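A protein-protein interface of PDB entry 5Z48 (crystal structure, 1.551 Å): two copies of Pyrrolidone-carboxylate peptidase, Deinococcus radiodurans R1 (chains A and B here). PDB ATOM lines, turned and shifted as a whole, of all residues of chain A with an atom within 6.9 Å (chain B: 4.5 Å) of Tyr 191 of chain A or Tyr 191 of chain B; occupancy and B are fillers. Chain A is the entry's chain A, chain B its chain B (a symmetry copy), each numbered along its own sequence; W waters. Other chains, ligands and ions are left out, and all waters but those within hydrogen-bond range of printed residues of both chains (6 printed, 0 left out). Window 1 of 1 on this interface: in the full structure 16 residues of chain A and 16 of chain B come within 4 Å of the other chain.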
ATOM      1  N   ARG A  77       8.947 -23.069  11.916  1.00  0.00           N
ATOM      2  CA  ARG A  77      10.236 -22.551  12.390  1.00  0.00           C
ATOM      3  C   ARG A  77      10.766 -23.407  13.547  1.00  0.00           C
ATOM      4  O   ARG A  77      10.006 -23.827  14.417  1.00  0.00           O
ATOM      5  CB  ARG A  77      10.111 -21.065  12.811  1.00  0.00           C
ATOM      6  CG  ARG A  77       9.715 -20.103  11.703  1.00  0.00           C
ATOM      7  CD  ARG A  77      10.010 -18.666  12.100  1.00  0.00           C
ATOM      8  NE  ARG A  77       9.504 -17.790  11.022  1.00  0.00           N
ATOM      9  CZ  ARG A  77       9.433 -16.452  11.123  1.00  0.00           C
ATOM     10  NH1 ARG A  77       9.835 -15.821  12.207  1.00  0.00           N
ATOM     11  NH2 ARG A  77       8.922 -15.736  10.119  1.00  0.00           N
ATOM     12  N   PRO A  78      12.074 -23.670  13.579  1.00  0.00           N
ATOM     13  CA  PRO A  78      12.639 -24.555  14.626  1.00  0.00           C
ATOM     14  C   PRO A  78      12.920 -23.865  15.958  1.00  0.00           C
ATOM     15  O   PRO A  78      13.003 -24.559  16.980  1.00  0.00           O
ATOM     16  CB  PRO A  78      13.956 -25.057  14.011  1.00  0.00           C
ATOM     17  CG  PRO A  78      14.355 -23.885  13.066  1.00  0.00           C
ATOM     18  CD  PRO A  78      13.010 -23.403  12.480  1.00  0.00           C
ATOM     19  N   GLN A  79      13.074 -22.540  15.998  1.00  0.00           N
ATOM     20  CA  GLN A  79      13.547 -21.851  17.198  1.00  0.00           C
ATOM     21  C   GLN A  79      12.783 -20.550  17.317  1.00  0.00           C
ATOM     22  O   GLN A  79      12.318 -19.999  16.303  1.00  0.00           O
ATOM     23  CB  GLN A  79      15.067 -21.573  17.126  1.00  0.00           C
ATOM     24  CG  GLN A  79      15.864 -22.873  16.895  1.00  0.00           C
ATOM     25  CD  GLN A  79      17.370 -22.642  16.631  1.00  0.00           C
ATOM     26  OE1 GLN A  79      17.824 -21.483  16.625  1.00  0.00           O
ATOM     27  NE2 GLN A  79      18.136 -23.736  16.457  1.00  0.00           N
ATOM     28  N   VAL A  80      12.675 -20.056  18.555  1.00  0.00           N
ATOM     29  CA  VAL A  80      12.076 -18.742  18.760  1.00  0.00           C
ATOM     30  C   VAL A  80      12.822 -17.683  17.947  1.00  0.00           C
ATOM     31  O   VAL A  80      14.060 -17.722  17.807  1.00  0.00           O
ATOM     32  CB  VAL A  80      12.007 -18.354  20.261  1.00  0.00           C
ATOM     33  CG1 VAL A  80      11.004 -19.224  20.985  1.00  0.00           C
ATOM     34  CG2 VAL A  80      13.351 -18.396  20.987  1.00  0.00           C
ATOM     35  N   GLU A 132      20.331 -20.994  27.653  1.00  0.00           N
ATOM     36  CA  GLU A 132      20.458 -22.179  26.787  1.00  0.00           C
ATOM     37  C   GLU A 132      19.287 -22.350  25.825  1.00  0.00           C
ATOM     38  O   GLU A 132      18.924 -23.490  25.484  1.00  0.00           O
ATOM     39  CB  GLU A 132      20.662 -23.457  27.602  1.00  0.00           C
ATOM     40  CG  GLU A 132      21.932 -23.360  28.451  1.00  0.00           C
ATOM     41  CD  GLU A 132      22.218 -24.552  29.301  1.00  0.00           C
ATOM     42  OE1 GLU A 132      23.182 -24.437  30.101  1.00  0.00           O
ATOM     43  OE2 GLU A 132      21.545 -25.609  29.160  1.00  0.00           O
ATOM     44  N   ILE A 133      18.772 -21.233  25.319  1.00  0.00           N
ATOM     45  CA  ILE A 133      17.674 -21.221  24.352  1.00  0.00           C
ATOM     46  C   ILE A 133      18.219 -20.736  23.016  1.00  0.00           C
ATOM     47  O   ILE A 133      18.636 -19.572  22.901  1.00  0.00           O
ATOM     48  CB  ILE A 133      16.514 -20.338  24.813  1.00  0.00           C
ATOM     49  CG1 ILE A 133      15.935 -20.913  26.113  1.00  0.00           C
ATOM     50  CG2 ILE A 133      15.454 -20.265  23.719  1.00  0.00           C
ATOM     51  CD1 ILE A 133      15.025 -19.942  26.825  1.00  0.00           C
ATOM     52  N   PRO A 134      18.219 -21.594  22.004  1.00  0.00           N
ATOM     53  CA  PRO A 134      18.575 -21.171  20.644  1.00  0.00           C
ATOM     54  C   PRO A 134      17.547 -20.193  20.104  1.00  0.00           C
ATOM     55  O   PRO A 134      16.351 -20.344  20.359  1.00  0.00           O
ATOM     56  CB  PRO A 134      18.550 -22.492  19.851  1.00  0.00           C
ATOM     57  CG  PRO A 134      18.497 -23.593  20.824  1.00  0.00           C
ATOM     58  CD  PRO A 134      17.904 -23.032  22.102  1.00  0.00           C
ATOM     59  N   GLY A 135      18.011 -19.174  19.369  1.00  0.00           N
ATOM     60  CA  GLY A 135      17.065 -18.218  18.797  1.00  0.00           C
ATOM     61  C   GLY A 135      17.776 -17.240  17.883  1.00  0.00           C
ATOM     62  O   GLY A 135      19.009 -17.169  17.869  1.00  0.00           O
ATOM     63  N   PRO A 173       7.871 -21.525  17.758  1.00  0.00           N
ATOM     64  CA  PRO A 173       7.557 -22.769  17.059  1.00  0.00           C
ATOM     65  C   PRO A 173       6.235 -23.391  17.476  1.00  0.00           C
ATOM     66  O   PRO A 173       5.623 -23.029  18.479  1.00  0.00           O
ATOM     67  CB  PRO A 173       8.710 -23.693  17.488  1.00  0.00           C
ATOM     68  CG  PRO A 173       9.885 -22.768  17.747  1.00  0.00           C
ATOM     69  CD  PRO A 173       9.188 -21.584  18.432  1.00  0.00           C
ATOM     70  N   ALA A 174       5.835 -24.401  16.692  1.00  0.00           N
ATOM     71  CA  ALA A 174       4.765 -25.306  17.120  1.00  0.00           C
ATOM     72  C   ALA A 174       5.084 -25.881  18.496  1.00  0.00           C
ATOM     73  O   ALA A 174       6.249 -26.103  18.826  1.00  0.00           O
ATOM     74  CB  ALA A 174       4.637 -26.453  16.107  1.00  0.00           C
ATOM     75  N   ASN A 175       4.055 -26.117  19.310  1.00  0.00           N
ATOM     76  CA  ASN A 175       4.218 -26.965  20.483  1.00  0.00           C
ATOM     77  C   ASN A 175       3.836 -28.393  20.093  1.00  0.00           C
ATOM     78  O   ASN A 175       3.573 -28.696  18.921  1.00  0.00           O
ATOM     79  CB  ASN A 175       3.406 -26.419  21.664  1.00  0.00           C
ATOM     80  CG  ASN A 175       1.897 -26.365  21.404  1.00  0.00           C
ATOM     81  OD1 ASN A 175       1.390 -26.876  20.401  1.00  0.00           O
ATOM     82  ND2 ASN A 175       1.155 -25.731  22.341  1.00  0.00           N
ATOM     83  N   ALA A 176       3.787 -29.303  21.079  1.00  0.00           N
ATOM     84  CA  ALA A 176       3.477 -30.695  20.747  1.00  0.00           C
ATOM     85  C   ALA A 176       2.078 -30.825  20.153  1.00  0.00           C
ATOM     86  O   ALA A 176       1.865 -31.603  19.205  1.00  0.00           O
ATOM     87  CB  ALA A 176       3.635 -31.579  21.997  1.00  0.00           C
ATOM     88  N   ALA A 177       1.099 -30.085  20.698  1.00  0.00           N
ATOM     89  CA  ALA A 177      -0.271 -30.185  20.199  1.00  0.00           C
ATOM     90  C   ALA A 177      -0.356 -29.782  18.735  1.00  0.00           C
ATOM     91  O   ALA A 177      -1.062 -30.441  17.949  1.00  0.00           O
ATOM     92  CB  ALA A 177      -1.201 -29.306  21.045  1.00  0.00           C
ATOM     93  N   VAL A 178       0.336 -28.693  18.352  1.00  0.00           N
ATOM     94  CA  VAL A 178       0.331 -28.288  16.948  1.00  0.00           C
ATOM     95  C   VAL A 178       0.969 -29.379  16.083  1.00  0.00           C
ATOM     96  O   VAL A 178       0.449 -29.732  15.015  1.00  0.00           O
ATOM     97  CB  VAL A 178       1.027 -26.922  16.789  1.00  0.00           C
ATOM     98  CG1 VAL A 178       1.259 -26.582  15.298  1.00  0.00           C
ATOM     99  CG2 VAL A 178       0.197 -25.821  17.506  1.00  0.00           C
ATOM    100  N   ALA A 179       2.111 -29.928  16.533  1.00  0.00           N
ATOM    101  CA  ALA A 179       2.822 -30.922  15.726  1.00  0.00           C
ATOM    102  C   ALA A 179       2.031 -32.215  15.593  1.00  0.00           C
ATOM    103  O   ALA A 179       2.089 -32.880  14.547  1.00  0.00           O
ATOM    104  CB  ALA A 179       4.207 -31.193  16.359  1.00  0.00           C
ATOM    105  N   LEU A 180       1.323 -32.625  16.661  1.00  0.00           N
ATOM    106  CA  LEU A 180       0.557 -33.877  16.655  1.00  0.00           C
ATOM    107  C   LEU A 180      -0.628 -33.858  15.700  1.00  0.00           C
ATOM    108  O   LEU A 180      -1.088 -34.927  15.310  1.00  0.00           O
ATOM    109  CB  LEU A 180       0.036 -34.203  18.059  1.00  0.00           C
ATOM    110  CG  LEU A 180       1.150 -34.643  18.995  1.00  0.00           C
ATOM    111  CD1 LEU A 180       0.643 -34.544  20.432  1.00  0.00           C
ATOM    112  CD2 LEU A 180       1.578 -36.086  18.640  1.00  0.00           C
ATOM    113  N   LEU A 189       6.536 -31.174  11.590  1.00  0.00           N
ATOM    114  CA  LEU A 189       6.935 -29.855  12.036  1.00  0.00           C
ATOM    115  C   LEU A 189       8.026 -29.946  13.094  1.00  0.00           C
ATOM    116  O   LEU A 189       7.907 -30.743  14.040  1.00  0.00           O
ATOM    117  CB  LEU A 189       5.745 -29.106  12.660  1.00  0.00           C
ATOM    118  CG  LEU A 189       4.633 -28.687  11.695  1.00  0.00           C
ATOM    119  CD1 LEU A 189       3.528 -28.063  12.527  1.00  0.00           C
ATOM    120  CD2 LEU A 189       5.190 -27.707  10.613  1.00  0.00           C
ATOM    121  N   PRO A 190       9.049 -29.105  13.022  1.00  0.00           N
ATOM    122  CA  PRO A 190       9.814 -28.797  14.231  1.00  0.00           C
ATOM    123  C   PRO A 190       8.849 -28.331  15.313  1.00  0.00           C
ATOM    124  O   PRO A 190       7.840 -27.676  15.039  1.00  0.00           O
ATOM    125  CB  PRO A 190      10.767 -27.672  13.792  1.00  0.00           C
ATOM    126  CG  PRO A 190      10.873 -27.788  12.300  1.00  0.00           C
ATOM    127  CD  PRO A 190       9.465 -28.271  11.874  1.00  0.00           C
ATOM    128  N   TYR A 191       9.160 -28.667  16.559  1.00  0.00           N
ATOM    129  CA  TYR A 191       8.318 -28.248  17.671  1.00  0.00           C
ATOM    130  C   TYR A 191       9.145 -28.113  18.943  1.00  0.00           C
ATOM    131  O   TYR A 191      10.298 -28.541  19.019  1.00  0.00           O
ATOM    132  CB  TYR A 191       7.160 -29.245  17.889  1.00  0.00           C
ATOM    133  CG  TYR A 191       7.545 -30.500  18.645  1.00  0.00           C
ATOM    134  CD1 TYR A 191       8.216 -31.547  18.007  1.00  0.00           C
ATOM    135  CD2 TYR A 191       7.239 -30.624  19.986  1.00  0.00           C
ATOM    136  CE1 TYR A 191       8.618 -32.690  18.724  1.00  0.00           C
ATOM    137  CE2 TYR A 191       7.627 -31.758  20.707  1.00  0.00           C
ATOM    138  CZ  TYR A 191       8.292 -32.787  20.075  1.00  0.00           C
ATOM    139  OH  TYR A 191       8.676 -33.889  20.805  1.00  0.00           O
ATOM    140  N   LEU A 192       8.538 -27.500  19.943  1.00  0.00           N
ATOM    141  CA  LEU A 192       9.120 -27.433  21.266  1.00  0.00           C
ATOM    142  C   LEU A 192       8.027 -27.742  22.269  1.00  0.00           C
ATOM    143  O   LEU A 192       6.866 -27.346  22.073  1.00  0.00           O
ATOM    144  CB  LEU A 192       9.725 -26.043  21.574  1.00  0.00           C
ATOM    145  CG  LEU A 192      10.905 -25.675  20.678  1.00  0.00           C
ATOM    146  CD1 LEU A 192      11.302 -24.194  20.882  1.00  0.00           C
ATOM    147  CD2 LEU A 192      12.066 -26.553  20.962  1.00  0.00           C
ATOM    148  N   PRO A 193       8.358 -28.402  23.379  1.00  0.00           N
ATOM    149  CA  PRO A 193       7.358 -28.500  24.444  1.00  0.00           C
ATOM    150  C   PRO A 193       6.907 -27.115  24.877  1.00  0.00           C
ATOM    151  O   PRO A 193       7.703 -26.157  24.887  1.00  0.00           O
ATOM    152  CB  PRO A 193       8.100 -29.217  25.578  1.00  0.00           C
ATOM    153  CG  PRO A 193       9.180 -30.037  24.828  1.00  0.00           C
ATOM    154  CD  PRO A 193       9.602 -29.088  23.733  1.00  0.00           C
ATOM    155  N   GLN A 194       5.625 -27.027  25.264  1.00  0.00           N
ATOM    156  CA  GLN A 194       5.117 -25.716  25.660  1.00  0.00           C
ATOM    157  C   GLN A 194       5.972 -25.085  26.766  1.00  0.00           C
ATOM    158  O   GLN A 194       6.179 -23.867  26.773  1.00  0.00           O
ATOM    159  CB  GLN A 194       3.652 -25.830  26.094  1.00  0.00           C
ATOM    160  CG  GLN A 194       3.089 -24.469  26.502  1.00  0.00           C
ATOM    161  CD  GLN A 194       3.001 -23.529  25.317  1.00  0.00           C
ATOM    162  OE1 GLN A 194       2.475 -23.918  24.256  1.00  0.00           O
ATOM    163  NE2 GLN A 194       3.463 -22.276  25.501  1.00  0.00           N
ATOM    164  N   GLU A 196       9.106 -25.078  27.227  1.00  0.00           N
ATOM    165  CA  GLU A 196      10.268 -24.412  26.615  1.00  0.00           C
ATOM    166  C   GLU A 196       9.858 -23.101  25.955  1.00  0.00           C
ATOM    167  O   GLU A 196      10.548 -22.082  26.102  1.00  0.00           O
ATOM    168  CB  GLU A 196      10.938 -25.354  25.617  1.00  0.00           C
ATOM    169  CG  GLU A 196      12.092 -24.729  24.804  1.00  0.00           C
ATOM    170  CD  GLU A 196      13.406 -24.609  25.540  1.00  0.00           C
ATOM    171  OE1 GLU A 196      13.482 -24.789  26.795  1.00  0.00           O
ATOM    172  OE2 GLU A 196      14.434 -24.369  24.850  1.00  0.00           O
ATOM    173  N   ILE A 197       8.724 -23.109  25.243  1.00  0.00           N
ATOM    174  CA  ILE A 197       8.203 -21.895  24.599  1.00  0.00           C
ATOM    175  C   ILE A 197       7.887 -20.837  25.643  1.00  0.00           C
ATOM    176  O   ILE A 197       8.275 -19.668  25.501  1.00  0.00           O
ATOM    177  CB  ILE A 197       6.966 -22.238  23.760  1.00  0.00           C
ATOM    178  CG1 ILE A 197       7.404 -23.163  22.615  1.00  0.00           C
ATOM    179  CG2 ILE A 197       6.314 -20.968  23.173  1.00  0.00           C
ATOM    180  CD1 ILE A 197       6.246 -23.728  21.779  1.00  0.00           C
ATOM    181  N   ARG A 199       9.025 -20.518  28.675  1.00  0.00           N
ATOM    182  CA  ARG A 199      10.274 -20.019  29.249  1.00  0.00           C
ATOM    183  C   ARG A 199      10.975 -19.029  28.315  1.00  0.00           C
ATOM    184  O   ARG A 199      11.507 -18.005  28.767  1.00  0.00           O
ATOM    185  CB  ARG A 199      11.194 -21.200  29.584  1.00  0.00           C
ATOM    186  CG  ARG A 199      12.393 -20.768  30.404  1.00  0.00           C
ATOM    187  CD  ARG A 199      13.171 -21.957  30.929  1.00  0.00           C
ATOM    188  NE  ARG A 199      13.761 -22.800  29.872  1.00  0.00           N
ATOM    189  CZ  ARG A 199      15.033 -22.711  29.468  1.00  0.00           C
ATOM    190  NH1 ARG A 199      15.873 -21.831  30.035  1.00  0.00           N
ATOM    191  NH2 ARG A 199      15.511 -23.512  28.528  1.00  0.00           N
ATOM    192  N   ALA A 200      10.970 -19.289  27.010  1.00  0.00           N
ATOM    193  CA  ALA A 200      11.596 -18.342  26.087  1.00  0.00           C
ATOM    194  C   ALA A 200      10.890 -16.993  26.119  1.00  0.00           C
ATOM    195  O   ALA A 200      11.534 -15.941  26.064  1.00  0.00           O
ATOM    196  CB  ALA A 200      11.580 -18.917  24.675  1.00  0.00           C
ATOM    197  N   PRO B  78      13.351 -33.241  13.102  1.00  0.00           N
ATOM    198  CA  PRO B  78      12.530 -32.482  14.077  1.00  0.00           C
ATOM    199  C   PRO B  78      11.928 -33.320  15.196  1.00  0.00           C
ATOM    200  O   PRO B  78      11.622 -32.761  16.263  1.00  0.00           O
ATOM    201  CB  PRO B  78      11.408 -31.876  13.204  1.00  0.00           C
ATOM    202  CG  PRO B  78      11.278 -32.883  12.045  1.00  0.00           C
ATOM    203  CD  PRO B  78      12.732 -33.279  11.763  1.00  0.00           C
ATOM    204  N   GLN B  79      11.783 -34.638  15.011  1.00  0.00           N
ATOM    205  CA  GLN B  79      11.010 -35.472  15.927  1.00  0.00           C
ATOM    206  C   GLN B  79      11.748 -36.791  16.094  1.00  0.00           C
ATOM    207  O   GLN B  79      12.492 -37.223  15.199  1.00  0.00           O
ATOM    208  CB  GLN B  79       9.559 -35.712  15.414  1.00  0.00           C
ATOM    209  CG  GLN B  79       8.801 -34.395  15.174  1.00  0.00           C
ATOM    210  CD  GLN B  79       7.429 -34.562  14.548  1.00  0.00           C
ATOM    211  OE1 GLN B  79       7.015 -35.694  14.277  1.00  0.00           O
ATOM    212  NE2 GLN B  79       6.692 -33.438  14.354  1.00  0.00           N
ATOM    213  N   ILE B 133       3.891 -37.061  22.363  1.00  0.00           N
ATOM    214  CA  ILE B 133       5.201 -36.960  21.706  1.00  0.00           C
ATOM    215  C   ILE B 133       5.011 -37.236  20.219  1.00  0.00           C
ATOM    216  O   ILE B 133       4.662 -38.370  19.845  1.00  0.00           O
ATOM    217  CB  ILE B 133       6.224 -37.932  22.321  1.00  0.00           C
ATOM    218  CG1 ILE B 133       6.448 -37.556  23.791  1.00  0.00           C
ATOM    219  CG2 ILE B 133       7.571 -37.878  21.571  1.00  0.00           C
ATOM    220  CD1 ILE B 133       7.208 -38.642  24.555  1.00  0.00           C
ATOM    221  N   PRO B 134       5.259 -36.247  19.343  1.00  0.00           N
ATOM    222  CA  PRO B 134       5.287 -36.495  17.888  1.00  0.00           C
ATOM    223  C   PRO B 134       6.442 -37.406  17.504  1.00  0.00           C
ATOM    224  O   PRO B 134       7.534 -37.304  18.061  1.00  0.00           O
ATOM    225  CB  PRO B 134       5.516 -35.097  17.298  1.00  0.00           C
ATOM    226  CG  PRO B 134       5.307 -34.113  18.361  1.00  0.00           C
ATOM    227  CD  PRO B 134       5.533 -34.841  19.697  1.00  0.00           C
ATOM    228  N   ALA B 174      18.568 -33.012  17.782  1.00  0.00           N
ATOM    229  CA  ALA B 174      19.469 -32.193  18.585  1.00  0.00           C
ATOM    230  C   ALA B 174      18.788 -31.804  19.893  1.00  0.00           C
ATOM    231  O   ALA B 174      17.580 -31.587  19.920  1.00  0.00           O
ATOM    232  CB  ALA B 174      19.822 -30.912  17.808  1.00  0.00           C
ATOM    233  N   ASN B 175      19.566 -31.716  20.980  1.00  0.00           N
ATOM    234  CA  ASN B 175      19.090 -31.005  22.153  1.00  0.00           C
ATOM    235  C   ASN B 175      19.560 -29.551  22.077  1.00  0.00           C
ATOM    236  O   ASN B 175      20.120 -29.113  21.061  1.00  0.00           O
ATOM    237  CB  ASN B 175      19.547 -31.715  23.427  1.00  0.00           C
ATOM    238  CG  ASN B 175      21.087 -31.761  23.567  1.00  0.00           C
ATOM    239  OD1 ASN B 175      21.828 -31.111  22.831  1.00  0.00           O
ATOM    240  ND2 ASN B 175      21.571 -32.561  24.537  1.00  0.00           N
ATOM    241  N   ALA B 176      19.332 -28.762  23.149  1.00  0.00           N
ATOM    242  CA  ALA B 176      19.715 -27.353  23.091  1.00  0.00           C
ATOM    243  C   ALA B 176      21.217 -27.194  22.888  1.00  0.00           C
ATOM    244  O   ALA B 176      21.655 -26.314  22.130  1.00  0.00           O
ATOM    245  CB  ALA B 176      19.277 -26.615  24.363  1.00  0.00           C
ATOM    246  N   ALA B 179      22.097 -27.597  19.311  1.00  0.00           N
ATOM    247  CA  ALA B 179      21.611 -26.498  18.471  1.00  0.00           C
ATOM    248  C   ALA B 179      22.392 -25.204  18.723  1.00  0.00           C
ATOM    249  O   ALA B 179      22.606 -24.407  17.796  1.00  0.00           O
ATOM    250  CB  ALA B 179      20.100 -26.282  18.718  1.00  0.00           C
ATOM    251  N   LEU B 189      19.094 -25.599  13.615  1.00  0.00           N
ATOM    252  CA  LEU B 189      18.607 -26.969  13.744  1.00  0.00           C
ATOM    253  C   LEU B 189      17.278 -27.000  14.485  1.00  0.00           C
ATOM    254  O   LEU B 189      17.134 -26.333  15.518  1.00  0.00           O
ATOM    255  CB  LEU B 189      19.599 -27.835  14.532  1.00  0.00           C
ATOM    256  CG  LEU B 189      20.944 -28.134  13.857  1.00  0.00           C
ATOM    257  CD1 LEU B 189      21.796 -28.884  14.888  1.00  0.00           C
ATOM    258  CD2 LEU B 189      20.707 -28.969  12.570  1.00  0.00           C
ATOM    259  N   PRO B 190      16.304 -27.795  14.056  1.00  0.00           N
ATOM    260  CA  PRO B 190      15.268 -28.232  14.990  1.00  0.00           C
ATOM    261  C   PRO B 190      15.924 -28.873  16.204  1.00  0.00           C
ATOM    262  O   PRO B 190      16.956 -29.558  16.096  1.00  0.00           O
ATOM    263  CB  PRO B 190      14.455 -29.260  14.188  1.00  0.00           C
ATOM    264  CG  PRO B 190      14.737 -28.959  12.727  1.00  0.00           C
ATOM    265  CD  PRO B 190      16.200 -28.482  12.759  1.00  0.00           C
ATOM    266  N   TYR B 191      15.311 -28.687  17.377  1.00  0.00           N
ATOM    267  CA  TYR B 191      15.871 -29.265  18.587  1.00  0.00           C
ATOM    268  C   TYR B 191      14.750 -29.557  19.575  1.00  0.00           C
ATOM    269  O   TYR B 191      13.608 -29.141  19.385  1.00  0.00           O
ATOM    270  CB  TYR B 191      16.915 -28.325  19.228  1.00  0.00           C
ATOM    271  CG  TYR B 191      16.300 -27.173  20.017  1.00  0.00           C
ATOM    272  CD1 TYR B 191      15.783 -26.040  19.372  1.00  0.00           C
ATOM    273  CD2 TYR B 191      16.224 -27.235  21.406  1.00  0.00           C
ATOM    274  CE1 TYR B 191      15.219 -24.996  20.105  1.00  0.00           C
ATOM    275  CE2 TYR B 191      15.644 -26.204  22.147  1.00  0.00           C
ATOM    276  CZ  TYR B 191      15.145 -25.097  21.501  1.00  0.00           C
ATOM    277  OH  TYR B 191      14.580 -24.107  22.266  1.00  0.00           O
ATOM    278  N   LEU B 192      15.075 -30.315  20.615  1.00  0.00           N
ATOM    279  CA  LEU B 192      14.149 -30.566  21.721  1.00  0.00           C
ATOM    280  C   LEU B 192      14.932 -30.423  23.012  1.00  0.00           C
ATOM    281  O   LEU B 192      16.107 -30.789  23.049  1.00  0.00           O
ATOM    282  CB  LEU B 192      13.543 -31.981  21.679  1.00  0.00           C
ATOM    283  CG  LEU B 192      12.671 -32.169  20.469  1.00  0.00           C
ATOM    284  CD1 LEU B 192      12.296 -33.641  20.417  1.00  0.00           C
ATOM    285  CD2 LEU B 192      11.445 -31.283  20.551  1.00  0.00           C
ATOM    286  N   PRO B 193      14.333 -29.899  24.079  1.00  0.00           N
ATOM    287  CA  PRO B 193      15.035 -29.941  25.366  1.00  0.00           C
ATOM    288  C   PRO B 193      15.392 -31.375  25.702  1.00  0.00           C
ATOM    289  O   PRO B 193      14.646 -32.312  25.380  1.00  0.00           O
ATOM    290  CB  PRO B 193      14.009 -29.391  26.367  1.00  0.00           C
ATOM    291  CG  PRO B 193      13.074 -28.513  25.472  1.00  0.00           C
ATOM    292  CD  PRO B 193      12.979 -29.336  24.218  1.00  0.00           C
ATOM    293  N   GLU B 196      12.675 -33.676  27.141  1.00  0.00           N
ATOM    294  CA  GLU B 196      11.728 -34.257  26.182  1.00  0.00           C
ATOM    295  C   GLU B 196      12.319 -35.472  25.475  1.00  0.00           C
ATOM    296  O   GLU B 196      11.633 -36.479  25.281  1.00  0.00           O
ATOM    297  CB  GLU B 196      11.321 -33.160  25.195  1.00  0.00           C
ATOM    298  CG  GLU B 196      10.442 -33.660  23.998  1.00  0.00           C
ATOM    299  CD  GLU B 196       8.983 -33.882  24.347  1.00  0.00           C
ATOM    300  OE1 GLU B 196       8.617 -33.856  25.561  1.00  0.00           O
ATOM    301  OE2 GLU B 196       8.135 -33.996  23.407  1.00  0.00           O
HETATM  302  O   HOH W   1      11.755 -30.052  16.753  1.00  0.00           O
HETATM  303  O   HOH W   2      12.733 -27.277  17.052  1.00  0.00           O
HETATM  304  O   HOH W   3      20.889 -24.157  15.622  1.00  0.00           O
HETATM  305  O   HOH W   4       9.642 -35.942  18.952  1.00  0.00           O
HETATM  306  O   HOH W   5      14.050 -21.830  20.458  1.00  0.00           O
HETATM  307  O   HOH W   6       4.355 -32.854  12.807  1.00  0.00           O
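Water W6 lies within hydrogen-bond range of O of Ala 179 of chain A, NE2 of Gln 79 of chain B and N of Leu 189 of chain A.
Tyr 191 of chain A touches just these residues of chain B: Pro 78, Gln 79, Pro 134, Tyr 191, Leu 192 and Glu 196. Of the printed residues of chain A, Pro 190 of chain B touches Pro 78. Of the printed residues of chain B, Gln 79 of chain A touches Ala 179, Leu 189 and Tyr 191. The nearest printed residue of chain B that does not touch Leu 189 of chain A is Pro 134 of chain B (5.9 Å).
NE2 of Gln 79 of chain A is in hydrogen-bond range of O of Leu 189 of chain B (2.9 Å). The backbone carbonyl oxygen of Leu 189 of chain A sits at hydrogen-bond distance from the side-chain amide nitrogen of Gln 79 of chain B, 3.0 Å away. OH of Tyr 191 of chain A is in hydrogen-bond range of OE2 of Glu 196 of chain B (2.7 Å). The side-chain carboxylate (OE2) of Glu 196 of chain A lies within hydrogen-bond range of the side-chain hydroxyl (OH) of Tyr 191 of chain B (2.6 Å). The backbone carbonyl oxygen (O) of Tyr 191 of chain A lies close to the backbone carbonyl oxygen (O) of Tyr 191 of chain B (3.4 Å).
Printed residues of chain B that touch a printed residue of chain A: Pro 78, Gln 79, Ile 133, Pro 134, Ala 176, Ala 179, Leu 189, Pro 190, Tyr 191, Leu 192, Pro 193 and Glu 196. Hydrophobic or aromatic side chains of chain B within 4 Å of the printed part of chain A: Pro 78, Pro 134, Ala 176, Ala 179, Tyr 191, Leu 192 and Pro 193. Along chain A the printed residues that touch a printed residue of chain B span positions 78 to 196. Among the printed residues, 27 pairs touch across the chains. Among the printed residues, no Asp or Glu carboxylate lies within 4 Å of a Lys or Arg side-chain nitrogen of the other chain.
Tyr 191 of chain A touches its own counterpart, Tyr 191 of chain B. Pro 193 of chain A touches Glu 196 of chain B, and with the chains exchanged Glu 196 of chain A touches Pro 193 of chain B.
O of Ala 174 of chain A is in hydrogen-bond range of N of Leu 192 of chain A, 2.9 Å away. The side-chain carboxylate (OE1) of Glu 196 of chain A is in salt-bridge range of the guanidinium group (NH2) of Arg 199 of chain A (3.0 Å).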
